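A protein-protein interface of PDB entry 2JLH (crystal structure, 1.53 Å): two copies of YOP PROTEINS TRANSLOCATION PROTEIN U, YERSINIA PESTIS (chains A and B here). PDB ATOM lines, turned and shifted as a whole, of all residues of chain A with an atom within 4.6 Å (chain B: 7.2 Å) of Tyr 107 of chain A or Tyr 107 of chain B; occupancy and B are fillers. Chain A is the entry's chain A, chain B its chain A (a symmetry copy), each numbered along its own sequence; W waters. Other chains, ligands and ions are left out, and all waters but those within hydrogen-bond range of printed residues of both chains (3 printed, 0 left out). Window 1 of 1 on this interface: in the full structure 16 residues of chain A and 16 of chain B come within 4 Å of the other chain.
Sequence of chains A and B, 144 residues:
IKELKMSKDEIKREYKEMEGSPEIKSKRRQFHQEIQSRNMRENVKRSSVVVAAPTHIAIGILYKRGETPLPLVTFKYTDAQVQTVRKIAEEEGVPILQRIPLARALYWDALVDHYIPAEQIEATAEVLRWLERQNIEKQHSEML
The side-chain hydroxyl (OH) of Tyr 107 of chain B is in hydrogen-bond range of the side-chain hydroxyl (OH) of Tyr 107 of chain A, at 2.4 Å.
O of Tyr 107 of chain A sits at hydrogen-bond distance from NZ of Lys 76 of chain A (2.8 Å).
NE of Arg 29 of chain B sits at hydrogen-bond distance from O of Trp 108 of chain B (3.2 Å).
The backbone carbonyl oxygen (O) of His 56 of chain B sits at hydrogen-bond distance from the backbone NH (N) of Asp 79 of chain B, at 3.0 Å.
NZ of Lys 76 of chain B sits at hydrogen-bond distance from O of Tyr 107 of chain B, 2.8 Å away.
CH2 of Trp 108 of chain B touches CD1 of Ile 57 of chain A (3.3 Å).
Trp 108 of chain B touches Arg 104 of chain A (NE1 to NE, 3.9 Å).
Trp 108 of chain B touches Tyr 107 of chain A.
His 56 of chain B touches Trp 108 of chain A.
CH2 of Trp 108 of chain A touches CD1 of Ile 57 of chain B, at 3.3 Å.
Arg 104 of chain B touches Trp 108 of chain A.
CH2 of Trp 108 of chain A touches CD2 of Tyr 107 of chain B, at 3.5 Å.
Trp 108 of chain A touches Trp 108 of chain B (CZ2 to CZ2, 3.2 Å).
His 56 of chain B touches Asp 109 of chain A (NE2 to OD1, 3.5 Å).
Of the printed residues of chain B, Ile 57 of chain A touches Trp 108.
Of chain B, only Tyr 107 and Trp 108 come within 4 Å of Tyr 107 of chain A.
Printed residues of chain B within 4 Å of Asp 109 of chain A: His 56.
Printed residues of chain A within 4 Å of Ile 57 of chain B: Trp 108.
Asp 79 of chain B touches none of the printed residues of chain A.
Tyr 107 of chain B touches just these residues of chain A: Tyr 107 and Trp 108.
Of the 22 printed residues of chain B, 5 touch a printed residue of chain A.
Printed residues of chain B that touch a printed residue of chain A: His 56, Ile 57, Arg 104, Tyr 107 and Trp 108.
Hydrophobic or aromatic side chains of chain B that line the printed part of chain A: His 56, Ile 57, Tyr 107 and Trp 108.
Printed residues of chain A that touch a printed residue of chain B: Ile 57, Arg 104, Tyr 107, Trp 108 and Asp 109.
Among the printed residues, 10 pairs touch across the chains.
Ile 57 of chain A touches Trp 108 of chain B, and with the chains exchanged Trp 108 of chain A touches Ile 57 of chain B.
Tyr 107 of chain B touches its own counterpart, Tyr 107 of chain A.
Tyr 107 of chain A touches Trp 108 of chain B, and with the chains exchanged Trp 108 of chain A touches Tyr 107 of chain B.
Trp 108 of chain B touches its own counterpart, Trp 108 of chain A.
Of the 10 pairs that touch across the chains among the printed residues, 8 have their exchanged pair printed and touching as well.
Water W1 lies within hydrogen-bond range of the side-chain carboxylate of Asp 79 of chain B (2.6 Å) and the backbone carbonyl oxygen of Trp 108 of chain A (2.6 Å).
Water W3 lies within hydrogen-bond range of the side-chain carboxylate of Asp 79 of chain B (2.7 Å), the side-chain amino group of Lys 76 of chain A (3.0 Å) and the backbone carbonyl oxygen of Tyr 107 of chain A (3.0 Å).
Water W2 bridges OD1 of Asp 109 of chain A (2.9 Å) and NE2 of His 56 of chain B (3.4 Å).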
ATOM      1  N   ILE A  57       9.190   7.890  25.602  1.00  0.00           N
ATOM      2  CA  ILE A  57       9.484   8.064  27.046  1.00  0.00           C
ATOM      3  C   ILE A  57       9.465   9.509  27.475  1.00  0.00           C
ATOM      4  O   ILE A  57       9.963  10.359  26.734  1.00  0.00           O
ATOM      5  CB  ILE A  57      10.948   7.609  27.413  1.00  0.00           C
ATOM      6  CG1 ILE A  57      11.252   6.226  26.931  1.00  0.00           C
ATOM      7  CG2 ILE A  57      11.161   7.703  28.957  1.00  0.00           C
ATOM      8  CD1 ILE A  57      12.733   5.921  27.056  1.00  0.00           C
ATOM      9  N   ILE A  59      10.522  11.517  31.163  1.00  0.00           N
ATOM     10  CA  ILE A  59      10.998  11.388  32.539  1.00  0.00           C
ATOM     11  C   ILE A  59      11.055  12.784  33.160  1.00  0.00           C
ATOM     12  O   ILE A  59      11.658  13.687  32.562  1.00  0.00           O
ATOM     13  CB  ILE A  59      12.449  10.826  32.656  1.00  0.00           C
ATOM     14  CG1 ILE A  59      12.654   9.557  31.782  1.00  0.00           C
ATOM     15  CG2 ILE A  59      12.807  10.626  34.115  1.00  0.00           C
ATOM     16  CD1 ILE A  59      11.941   8.303  32.285  1.00  0.00           C
ATOM     17  N   LYS A  76       7.665   8.823  35.367  1.00  0.00           N
ATOM     18  CA  LYS A  76       7.929   8.170  34.093  1.00  0.00           C
ATOM     19  C   LYS A  76       6.599   7.901  33.388  1.00  0.00           C
ATOM     20  O   LYS A  76       5.689   7.343  33.979  1.00  0.00           O
ATOM     21  CB  LYS A  76       8.603   6.809  34.278  1.00  0.00           C
ATOM     22  CG  LYS A  76       9.879   6.810  35.115  1.00  0.00           C
ATOM     23  CD  LYS A  76      10.496   5.415  35.185  1.00  0.00           C
ATOM     24  CE  LYS A  76      11.737   5.349  36.050  1.00  0.00           C
ATOM     25  NZ  LYS A  76      12.206   3.942  36.212  1.00  0.00           N
ATOM     26  N   THR A  78       5.029   6.829  29.218  1.00  0.00           N
ATOM     27  CA  THR A  78       5.484   6.258  27.959  1.00  0.00           C
ATOM     28  C   THR A  78       4.416   6.256  26.891  1.00  0.00           C
ATOM     29  O   THR A  78       3.254   6.549  27.114  1.00  0.00           O
ATOM     30  CB  THR A  78       5.916   4.831  28.096  1.00  0.00           C
ATOM     31  OG1 THR A  78       4.764   4.074  28.458  1.00  0.00           O
ATOM     32  CG2 THR A  78       7.018   4.639  29.188  1.00  0.00           C
ATOM     33  N   ALA A 103      16.948   9.569  28.762  1.00  0.00           N
ATOM     34  CA  ALA A 103      15.607   9.127  29.042  1.00  0.00           C
ATOM     35  C   ALA A 103      15.505   7.630  29.159  1.00  0.00           C
ATOM     36  O   ALA A 103      14.877   7.118  30.075  1.00  0.00           O
ATOM     37  CB  ALA A 103      14.655   9.641  27.960  1.00  0.00           C
ATOM     38  N   ARG A 104      16.121   6.907  28.223  1.00  0.00           N
ATOM     39  CA  ARG A 104      16.147   5.445  28.309  1.00  0.00           C
ATOM     40  C   ARG A 104      16.847   4.959  29.567  1.00  0.00           C
ATOM     41  O   ARG A 104      16.317   4.065  30.275  1.00  0.00           O
ATOM     42  CB  ARG A 104      16.793   4.864  27.064  1.00  0.00           C
ATOM     43  CG  ARG A 104      16.006   4.990  25.797  1.00  0.00           C
ATOM     44  CD  ARG A 104      16.773   4.507  24.607  1.00  0.00           C
ATOM     45  NE  ARG A 104      15.906   4.504  23.444  1.00  0.00           N
ATOM     46  CZ  ARG A 104      16.300   4.247  22.212  1.00  0.00           C
ATOM     47  NH1 ARG A 104      17.569   3.984  21.955  1.00  0.00           N
ATOM     48  NH2 ARG A 104      15.397   4.288  21.228  1.00  0.00           N
ATOM     49  N   ALA A 105      17.993   5.559  29.867  1.00  0.00           N
ATOM     50  CA  ALA A 105      18.726   5.094  31.035  1.00  0.00           C
ATOM     51  C   ALA A 105      17.964   5.313  32.334  1.00  0.00           C
ATOM     52  O   ALA A 105      17.937   4.445  33.245  1.00  0.00           O
ATOM     53  CB  ALA A 105      20.059   5.780  31.101  1.00  0.00           C
ATOM     54  N   LEU A 106      17.339   6.476  32.460  1.00  0.00           N
ATOM     55  CA  LEU A 106      16.516   6.744  33.623  1.00  0.00           C
ATOM     56  C   LEU A 106      15.295   5.835  33.666  1.00  0.00           C
ATOM     57  O   LEU A 106      14.869   5.344  34.707  1.00  0.00           O
ATOM     58  CB  LEU A 106      16.091   8.207  33.670  1.00  0.00           C
ATOM     59  CG  LEU A 106      17.239   9.184  33.906  1.00  0.00           C
ATOM     60  CD1 LEU A 106      16.719  10.638  33.719  1.00  0.00           C
ATOM     61  CD2 LEU A 106      17.869   8.992  35.305  1.00  0.00           C
ATOM     62  N   TYR A 107      14.692   5.589  32.509  1.00  0.00           N
ATOM     63  CA  TYR A 107      13.564   4.694  32.471  1.00  0.00           C
ATOM     64  C   TYR A 107      13.917   3.323  33.069  1.00  0.00           C
ATOM     65  O   TYR A 107      13.160   2.749  33.872  1.00  0.00           O
ATOM     66  CB  TYR A 107      13.025   4.514  31.035  1.00  0.00           C
ATOM     67  CG  TYR A 107      11.744   3.751  30.968  1.00  0.00           C
ATOM     68  CD1 TYR A 107      10.552   4.381  31.230  1.00  0.00           C
ATOM     69  CD2 TYR A 107      11.738   2.390  30.721  1.00  0.00           C
ATOM     70  CE1 TYR A 107       9.339   3.646  31.215  1.00  0.00           C
ATOM     71  CE2 TYR A 107      10.555   1.669  30.676  1.00  0.00           C
ATOM     72  CZ  TYR A 107       9.377   2.304  30.964  1.00  0.00           C
ATOM     73  OH  TYR A 107       8.176   1.547  30.965  1.00  0.00           O
ATOM     74  N   TRP A 108      15.054   2.777  32.640  1.00  0.00           N
ATOM     75  CA  TRP A 108      15.439   1.440  33.096  1.00  0.00           C
ATOM     76  C   TRP A 108      15.854   1.403  34.549  1.00  0.00           C
ATOM     77  O   TRP A 108      15.542   0.429  35.238  1.00  0.00           O
ATOM     78  CB  TRP A 108      16.536   0.808  32.241  1.00  0.00           C
ATOM     79  CG  TRP A 108      16.165   0.593  30.777  1.00  0.00           C
ATOM     80  CD1 TRP A 108      16.872   1.049  29.691  1.00  0.00           C
ATOM     81  CD2 TRP A 108      14.988  -0.036  30.259  1.00  0.00           C
ATOM     82  NE1 TRP A 108      16.240   0.686  28.537  1.00  0.00           N
ATOM     83  CE2 TRP A 108      15.073   0.057  28.841  1.00  0.00           C
ATOM     84  CE3 TRP A 108      13.908  -0.700  30.834  1.00  0.00           C
ATOM     85  CZ2 TRP A 108      14.102  -0.527  28.007  1.00  0.00           C
ATOM     86  CZ3 TRP A 108      12.898  -1.218  29.974  1.00  0.00           C
ATOM     87  CH2 TRP A 108      13.025  -1.112  28.603  1.00  0.00           C
ATOM     88  N   ASP A 109      16.622   2.390  34.997  1.00  0.00           N
ATOM     89  CA  ASP A 109      17.345   2.280  36.261  1.00  0.00           C
ATOM     90  C   ASP A 109      16.911   3.204  37.369  1.00  0.00           C
ATOM     91  O   ASP A 109      17.226   2.912  38.531  1.00  0.00           O
ATOM     92  CB  ASP A 109      18.848   2.541  36.106  1.00  0.00           C
ATOM     93  CG  ASP A 109      19.570   1.640  35.101  1.00  0.00           C
ATOM     94  OD1 ASP A 109      19.172   0.525  34.727  1.00  0.00           O
ATOM     95  OD2 ASP A 109      20.694   2.100  34.721  1.00  0.00           O
ATOM     96  N   ARG B  29       0.327   1.213  20.391  1.00  0.00           N
ATOM     97  CA  ARG B  29       1.030   0.416  21.402  1.00  0.00           C
ATOM     98  C   ARG B  29       0.313   0.467  22.721  1.00  0.00           C
ATOM     99  O   ARG B  29       0.000  -0.565  23.330  1.00  0.00           O
ATOM    100  CB  ARG B  29       2.495   0.852  21.574  1.00  0.00           C
ATOM    101  CG  ARG B  29       3.332   0.517  20.355  1.00  0.00           C
ATOM    102  CD  ARG B  29       4.837   0.697  20.645  1.00  0.00           C
ATOM    103  NE  ARG B  29       5.140   2.070  21.042  1.00  0.00           N
ATOM    104  CZ  ARG B  29       5.499   3.080  20.248  1.00  0.00           C
ATOM    105  NH1 ARG B  29       5.543   2.970  18.955  1.00  0.00           N
ATOM    106  NH2 ARG B  29       5.716   4.247  20.786  1.00  0.00           N
ATOM    107  N   GLN B  33      -1.797  -2.718  24.427  1.00  0.00           N
ATOM    108  CA  GLN B  33      -1.360  -3.145  25.751  1.00  0.00           C
ATOM    109  C   GLN B  33      -2.537  -3.124  26.730  1.00  0.00           C
ATOM    110  O   GLN B  33      -2.801  -4.082  27.484  1.00  0.00           O
ATOM    111  CB  GLN B  33      -0.223  -2.247  26.201  1.00  0.00           C
ATOM    112  CG  GLN B  33       0.463  -2.668  27.510  1.00  0.00           C
ATOM    113  CD  GLN B  33       1.361  -3.898  27.318  1.00  0.00           C
ATOM    114  OE1 GLN B  33       2.410  -3.853  26.687  1.00  0.00           O
ATOM    115  NE2 GLN B  33       0.866  -5.018  27.807  1.00  0.00           N
ATOM    116  N   HIS B  56      14.773  -6.493  34.166  1.00  0.00           N
ATOM    117  CA  HIS B  56      14.289  -5.293  33.497  1.00  0.00           C
ATOM    118  C   HIS B  56      13.111  -5.549  32.576  1.00  0.00           C
ATOM    119  O   HIS B  56      12.083  -4.871  32.667  1.00  0.00           O
ATOM    120  CB  HIS B  56      15.403  -4.575  32.754  1.00  0.00           C
ATOM    121  CG  HIS B  56      16.366  -3.896  33.662  1.00  0.00           C
ATOM    122  ND1 HIS B  56      17.493  -4.517  34.170  1.00  0.00           N
ATOM    123  CD2 HIS B  56      16.341  -2.668  34.216  1.00  0.00           C
ATOM    124  CE1 HIS B  56      18.142  -3.667  34.946  1.00  0.00           C
ATOM    125  NE2 HIS B  56      17.474  -2.529  34.966  1.00  0.00           N
ATOM    126  N   ILE B  57      13.264  -6.473  31.627  1.00  0.00           N
ATOM    127  CA  ILE B  57      12.250  -6.690  30.565  1.00  0.00           C
ATOM    128  C   ILE B  57      12.020  -8.150  30.269  1.00  0.00           C
ATOM    129  O   ILE B  57      12.989  -8.911  30.229  1.00  0.00           O
ATOM    130  CB  ILE B  57      12.715  -6.118  29.172  1.00  0.00           C
ATOM    131  CG1 ILE B  57      13.151  -4.691  29.260  1.00  0.00           C
ATOM    132  CG2 ILE B  57      11.565  -6.269  28.127  1.00  0.00           C
ATOM    133  CD1 ILE B  57      13.841  -4.254  27.981  1.00  0.00           C
ATOM    134  N   ALA B  58      10.767  -8.580  30.074  1.00  0.00           N
ATOM    135  CA  ALA B  58      10.512  -9.906  29.497  1.00  0.00           C
ATOM    136  C   ALA B  58       9.472  -9.697  28.420  1.00  0.00           C
ATOM    137  O   ALA B  58       8.439  -9.052  28.634  1.00  0.00           O
ATOM    138  CB  ALA B  58       9.971 -10.878  30.532  1.00  0.00           C
ATOM    139  N   ILE B  59       9.746 -10.232  27.228  1.00  0.00           N
ATOM    140  CA  ILE B  59       8.860 -10.128  26.070  1.00  0.00           C
ATOM    141  C   ILE B  59       8.510 -11.542  25.605  1.00  0.00           C
ATOM    142  O   ILE B  59       9.423 -12.352  25.396  1.00  0.00           O
ATOM    143  CB  ILE B  59       9.515  -9.438  24.833  1.00  0.00           C
ATOM    144  CG1 ILE B  59      10.232  -8.114  25.216  1.00  0.00           C
ATOM    145  CG2 ILE B  59       8.488  -9.279  23.729  1.00  0.00           C
ATOM    146  CD1 ILE B  59       9.302  -6.959  25.587  1.00  0.00           C
ATOM    147  N   VAL B  73       4.233 -10.857  19.209  1.00  0.00           N
ATOM    148  CA  VAL B  73       4.561 -10.499  20.574  1.00  0.00           C
ATOM    149  C   VAL B  73       3.327 -10.747  21.426  1.00  0.00           C
ATOM    150  O   VAL B  73       2.248 -10.184  21.140  1.00  0.00           O
ATOM    151  CB  VAL B  73       5.015  -9.050  20.733  1.00  0.00           C
ATOM    152  CG1 VAL B  73       5.155  -8.652  22.135  1.00  0.00           C
ATOM    153  CG2 VAL B  73       6.336  -8.838  19.947  1.00  0.00           C
ATOM    154  N   LYS B  76       4.432  -8.032  27.370  1.00  0.00           N
ATOM    155  CA  LYS B  76       5.571  -7.294  27.898  1.00  0.00           C
ATOM    156  C   LYS B  76       5.390  -7.117  29.406  1.00  0.00           C
ATOM    157  O   LYS B  76       4.345  -6.678  29.855  1.00  0.00           O
ATOM    158  CB  LYS B  76       5.663  -5.888  27.306  1.00  0.00           C
ATOM    159  CG  LYS B  76       5.679  -5.811  25.782  1.00  0.00           C
ATOM    160  CD  LYS B  76       5.832  -4.368  25.302  1.00  0.00           C
ATOM    161  CE  LYS B  76       5.799  -4.228  23.794  1.00  0.00           C
ATOM    162  NZ  LYS B  76       5.792  -2.794  23.386  1.00  0.00           N
ATOM    163  N   TYR B  77       6.425  -7.498  30.139  1.00  0.00           N
ATOM    164  CA  TYR B  77       6.449  -7.287  31.586  1.00  0.00           C
ATOM    165  C   TYR B  77       7.790  -6.667  31.952  1.00  0.00           C
ATOM    166  O   TYR B  77       8.771  -6.783  31.186  1.00  0.00           O
ATOM    167  CB  TYR B  77       6.258  -8.605  32.375  1.00  0.00           C
ATOM    168  CG  TYR B  77       4.892  -9.211  32.188  1.00  0.00           C
ATOM    169  CD1 TYR B  77       4.723 -10.391  31.520  1.00  0.00           C
ATOM    170  CD2 TYR B  77       3.775  -8.575  32.652  1.00  0.00           C
ATOM    171  CE1 TYR B  77       3.453 -10.924  31.320  1.00  0.00           C
ATOM    172  CE2 TYR B  77       2.512  -9.118  32.471  1.00  0.00           C
ATOM    173  CZ  TYR B  77       2.369 -10.266  31.777  1.00  0.00           C
ATOM    174  OH  TYR B  77       1.116 -10.825  31.565  1.00  0.00           O
ATOM    175  N   THR B  78       7.866  -5.990  33.094  1.00  0.00           N
ATOM    176  CA  THR B  78       9.106  -5.316  33.452  1.00  0.00           C
ATOM    177  C   THR B  78       9.397  -5.361  34.933  1.00  0.00           C
ATOM    178  O   THR B  78       8.595  -5.774  35.754  1.00  0.00           O
ATOM    179  CB  THR B  78       9.098  -3.864  33.089  1.00  0.00           C
ATOM    180  OG1 THR B  78       8.088  -3.238  33.877  1.00  0.00           O
ATOM    181  CG2 THR B  78       8.788  -3.624  31.576  1.00  0.00           C
ATOM    182  N   ASP B  79      10.640  -5.054  35.246  1.00  0.00           N
ATOM    183  CA  ASP B  79      11.175  -4.940  36.591  1.00  0.00           C
ATOM    184  C   ASP B  79      10.917  -6.249  37.337  1.00  0.00           C
ATOM    185  O   ASP B  79      11.256  -7.308  36.825  1.00  0.00           O
ATOM    186  CB  ASP B  79      10.677  -3.652  37.243  1.00  0.00           C
ATOM    187  CG  ASP B  79      11.293  -2.427  36.637  1.00  0.00           C
ATOM    188  OD1 ASP B  79      12.434  -2.546  36.194  1.00  0.00           O
ATOM    189  OD2 ASP B  79      10.629  -1.373  36.640  1.00  0.00           O
ATOM    190  N   PRO B 101      19.456  -6.452  23.637  1.00  0.00           N
ATOM    191  CA  PRO B 101      19.039  -5.533  22.596  1.00  0.00           C
ATOM    192  C   PRO B 101      17.673  -5.837  21.950  1.00  0.00           C
ATOM    193  O   PRO B 101      16.894  -4.907  21.694  1.00  0.00           O
ATOM    194  CB  PRO B 101      20.172  -5.598  21.594  1.00  0.00           C
ATOM    195  CG  PRO B 101      21.257  -6.297  22.238  1.00  0.00           C
ATOM    196  CD  PRO B 101      20.810  -6.971  23.452  1.00  0.00           C
ATOM    197  N   LEU B 102      17.381  -7.108  21.706  1.00  0.00           N
ATOM    198  CA  LEU B 102      16.094  -7.512  21.136  1.00  0.00           C
ATOM    199  C   LEU B 102      14.946  -7.208  22.082  1.00  0.00           C
ATOM    200  O   LEU B 102      13.904  -6.677  21.695  1.00  0.00           O
ATOM    201  CB  LEU B 102      16.105  -8.996  20.773  1.00  0.00           C
ATOM    202  CG  LEU B 102      14.784  -9.486  20.181  1.00  0.00           C
ATOM    203  CD1 LEU B 102      14.327  -8.658  18.923  1.00  0.00           C
ATOM    204  CD2 LEU B 102      14.875 -10.964  19.859  1.00  0.00           C
ATOM    205  N   ALA B 103      15.111  -7.570  23.358  1.00  0.00           N
ATOM    206  CA  ALA B 103      14.095  -7.271  24.332  1.00  0.00           C
ATOM    207  C   ALA B 103      13.800  -5.798  24.426  1.00  0.00           C
ATOM    208  O   ALA B 103      12.646  -5.394  24.457  1.00  0.00           O
ATOM    209  CB  ALA B 103      14.509  -7.817  25.699  1.00  0.00           C
ATOM    210  N   ARG B 104      14.847  -4.973  24.477  1.00  0.00           N
ATOM    211  CA  ARG B 104      14.654  -3.523  24.480  1.00  0.00           C
ATOM    212  C   ARG B 104      13.955  -3.037  23.221  1.00  0.00           C
ATOM    213  O   ARG B 104      12.992  -2.233  23.307  1.00  0.00           O
ATOM    214  CB  ARG B 104      15.986  -2.822  24.672  1.00  0.00           C
ATOM    215  CG  ARG B 104      16.610  -2.958  26.026  1.00  0.00           C
ATOM    216  CD  ARG B 104      17.973  -2.345  26.084  1.00  0.00           C
ATOM    217  NE  ARG B 104      18.454  -2.366  27.452  1.00  0.00           N
ATOM    218  CZ  ARG B 104      19.666  -2.011  27.829  1.00  0.00           C
ATOM    219  NH1 ARG B 104      20.558  -1.618  26.937  1.00  0.00           N
ATOM    220  NH2 ARG B 104      19.983  -2.088  29.125  1.00  0.00           N
ATOM    221  N   ALA B 105      14.400  -3.540  22.075  1.00  0.00           N
ATOM    222  CA  ALA B 105      13.797  -3.067  20.838  1.00  0.00           C
ATOM    223  C   ALA B 105      12.321  -3.422  20.729  1.00  0.00           C
ATOM    224  O   ALA B 105      11.471  -2.607  20.285  1.00  0.00           O
ATOM    225  CB  ALA B 105      14.546  -3.626  19.665  1.00  0.00           C
ATOM    226  N   LEU B 106      11.980  -4.643  21.118  1.00  0.00           N
ATOM    227  CA  LEU B 106      10.587  -5.045  21.133  1.00  0.00           C
ATOM    228  C   LEU B 106       9.788  -4.259  22.164  1.00  0.00           C
ATOM    229  O   LEU B 106       8.645  -3.862  21.957  1.00  0.00           O
ATOM    230  CB  LEU B 106      10.449  -6.543  21.384  1.00  0.00           C
ATOM    231  CG  LEU B 106      10.983  -7.418  20.255  1.00  0.00           C
ATOM    232  CD1 LEU B 106      10.987  -8.903  20.716  1.00  0.00           C
ATOM    233  CD2 LEU B 106      10.158  -7.238  18.959  1.00  0.00           C
ATOM    234  N   TYR B 107      10.387  -4.013  23.323  1.00  0.00           N
ATOM    235  CA  TYR B 107       9.709  -3.227  24.321  1.00  0.00           C
ATOM    236  C   TYR B 107       9.282  -1.861  23.763  1.00  0.00           C
ATOM    237  O   TYR B 107       8.144  -1.402  23.968  1.00  0.00           O
ATOM    238  CB  TYR B 107      10.580  -3.027  25.580  1.00  0.00           C
ATOM    239  CG  TYR B 107       9.853  -2.386  26.716  1.00  0.00           C
ATOM    240  CD1 TYR B 107       9.035  -3.137  27.523  1.00  0.00           C
ATOM    241  CD2 TYR B 107       9.927  -1.021  26.927  1.00  0.00           C
ATOM    242  CE1 TYR B 107       8.306  -2.519  28.571  1.00  0.00           C
ATOM    243  CE2 TYR B 107       9.239  -0.413  27.967  1.00  0.00           C
ATOM    244  CZ  TYR B 107       8.408  -1.169  28.747  1.00  0.00           C
ATOM    245  OH  TYR B 107       7.671  -0.529  29.778  1.00  0.00           O
ATOM    246  N   TRP B 108      10.216  -1.189  23.091  1.00  0.00           N
ATOM    247  CA  TRP B 108       9.926   0.154  22.585  1.00  0.00           C
ATOM    248  C   TRP B 108       8.951   0.157  21.428  1.00  0.00           C
ATOM    249  O   TRP B 108       8.116   1.062  21.349  1.00  0.00           O
ATOM    250  CB  TRP B 108      11.181   0.928  22.187  1.00  0.00           C
ATOM    251  CG  TRP B 108      12.166   1.180  23.325  1.00  0.00           C
ATOM    252  CD1 TRP B 108      13.499   0.848  23.327  1.00  0.00           C
ATOM    253  CD2 TRP B 108      11.882   1.720  24.620  1.00  0.00           C
ATOM    254  NE1 TRP B 108      14.068   1.207  24.514  1.00  0.00           N
ATOM    255  CE2 TRP B 108      13.111   1.707  25.340  1.00  0.00           C
ATOM    256  CE3 TRP B 108      10.746   2.251  25.224  1.00  0.00           C
ATOM    257  CZ2 TRP B 108      13.207   2.238  26.639  1.00  0.00           C
ATOM    258  CZ3 TRP B 108      10.847   2.714  26.567  1.00  0.00           C
ATOM    259  CH2 TRP B 108      12.062   2.689  27.225  1.00  0.00           C
ATOM    260  N   ASP B 109       9.100  -0.775  20.494  1.00  0.00           N
ATOM    261  CA  ASP B 109       8.445  -0.661  19.193  1.00  0.00           C
ATOM    262  C   ASP B 109       7.375  -1.676  18.885  1.00  0.00           C
ATOM    263  O   ASP B 109       6.562  -1.414  17.988  1.00  0.00           O
ATOM    264  CB  ASP B 109       9.431  -0.772  18.024  1.00  0.00           C
ATOM    265  CG  ASP B 109      10.578   0.243  18.035  1.00  0.00           C
ATOM    266  OD1 ASP B 109      10.561   1.333  18.630  1.00  0.00           O
ATOM    267  OD2 ASP B 109      11.558  -0.090  17.296  1.00  0.00           O
ATOM    268  N   ALA B 110       7.391  -2.843  19.515  1.00  0.00           N
ATOM    269  CA  ALA B 110       6.391  -3.872  19.171  1.00  0.00           C
ATOM    270  C   ALA B 110       5.015  -3.543  19.730  1.00  0.00           C
ATOM    271  O   ALA B 110       4.903  -2.892  20.803  1.00  0.00           O
ATOM    272  CB  ALA B 110       6.816  -5.239  19.669  1.00  0.00           C
ATOM    273  N   LEU B 111       3.983  -3.971  19.023  1.00  0.00           N
ATOM    274  CA  LEU B 111       2.636  -3.946  19.540  1.00  0.00           C
ATOM    275  C   LEU B 111       2.304  -5.313  20.075  1.00  0.00           C
ATOM    276  O   LEU B 111       2.478  -6.338  19.383  1.00  0.00           O
ATOM    277  CB  LEU B 111       1.602  -3.591  18.470  1.00  0.00           C
ATOM    278  CG  LEU B 111       1.491  -2.148  17.989  1.00  0.00           C
ATOM    279  CD1 LEU B 111       2.752  -1.660  17.310  1.00  0.00           C
ATOM    280  CD2 LEU B 111       0.227  -2.070  17.126  1.00  0.00           C
HETATM  281  O   HOH W   1      13.824  -1.363  34.400  1.00  0.00           O
HETATM  282  O   HOH W   2      20.011  -1.577  32.875  1.00  0.00           O
HETATM  283  O   HOH W   3      11.901   0.934  35.955  1.00  0.00           O
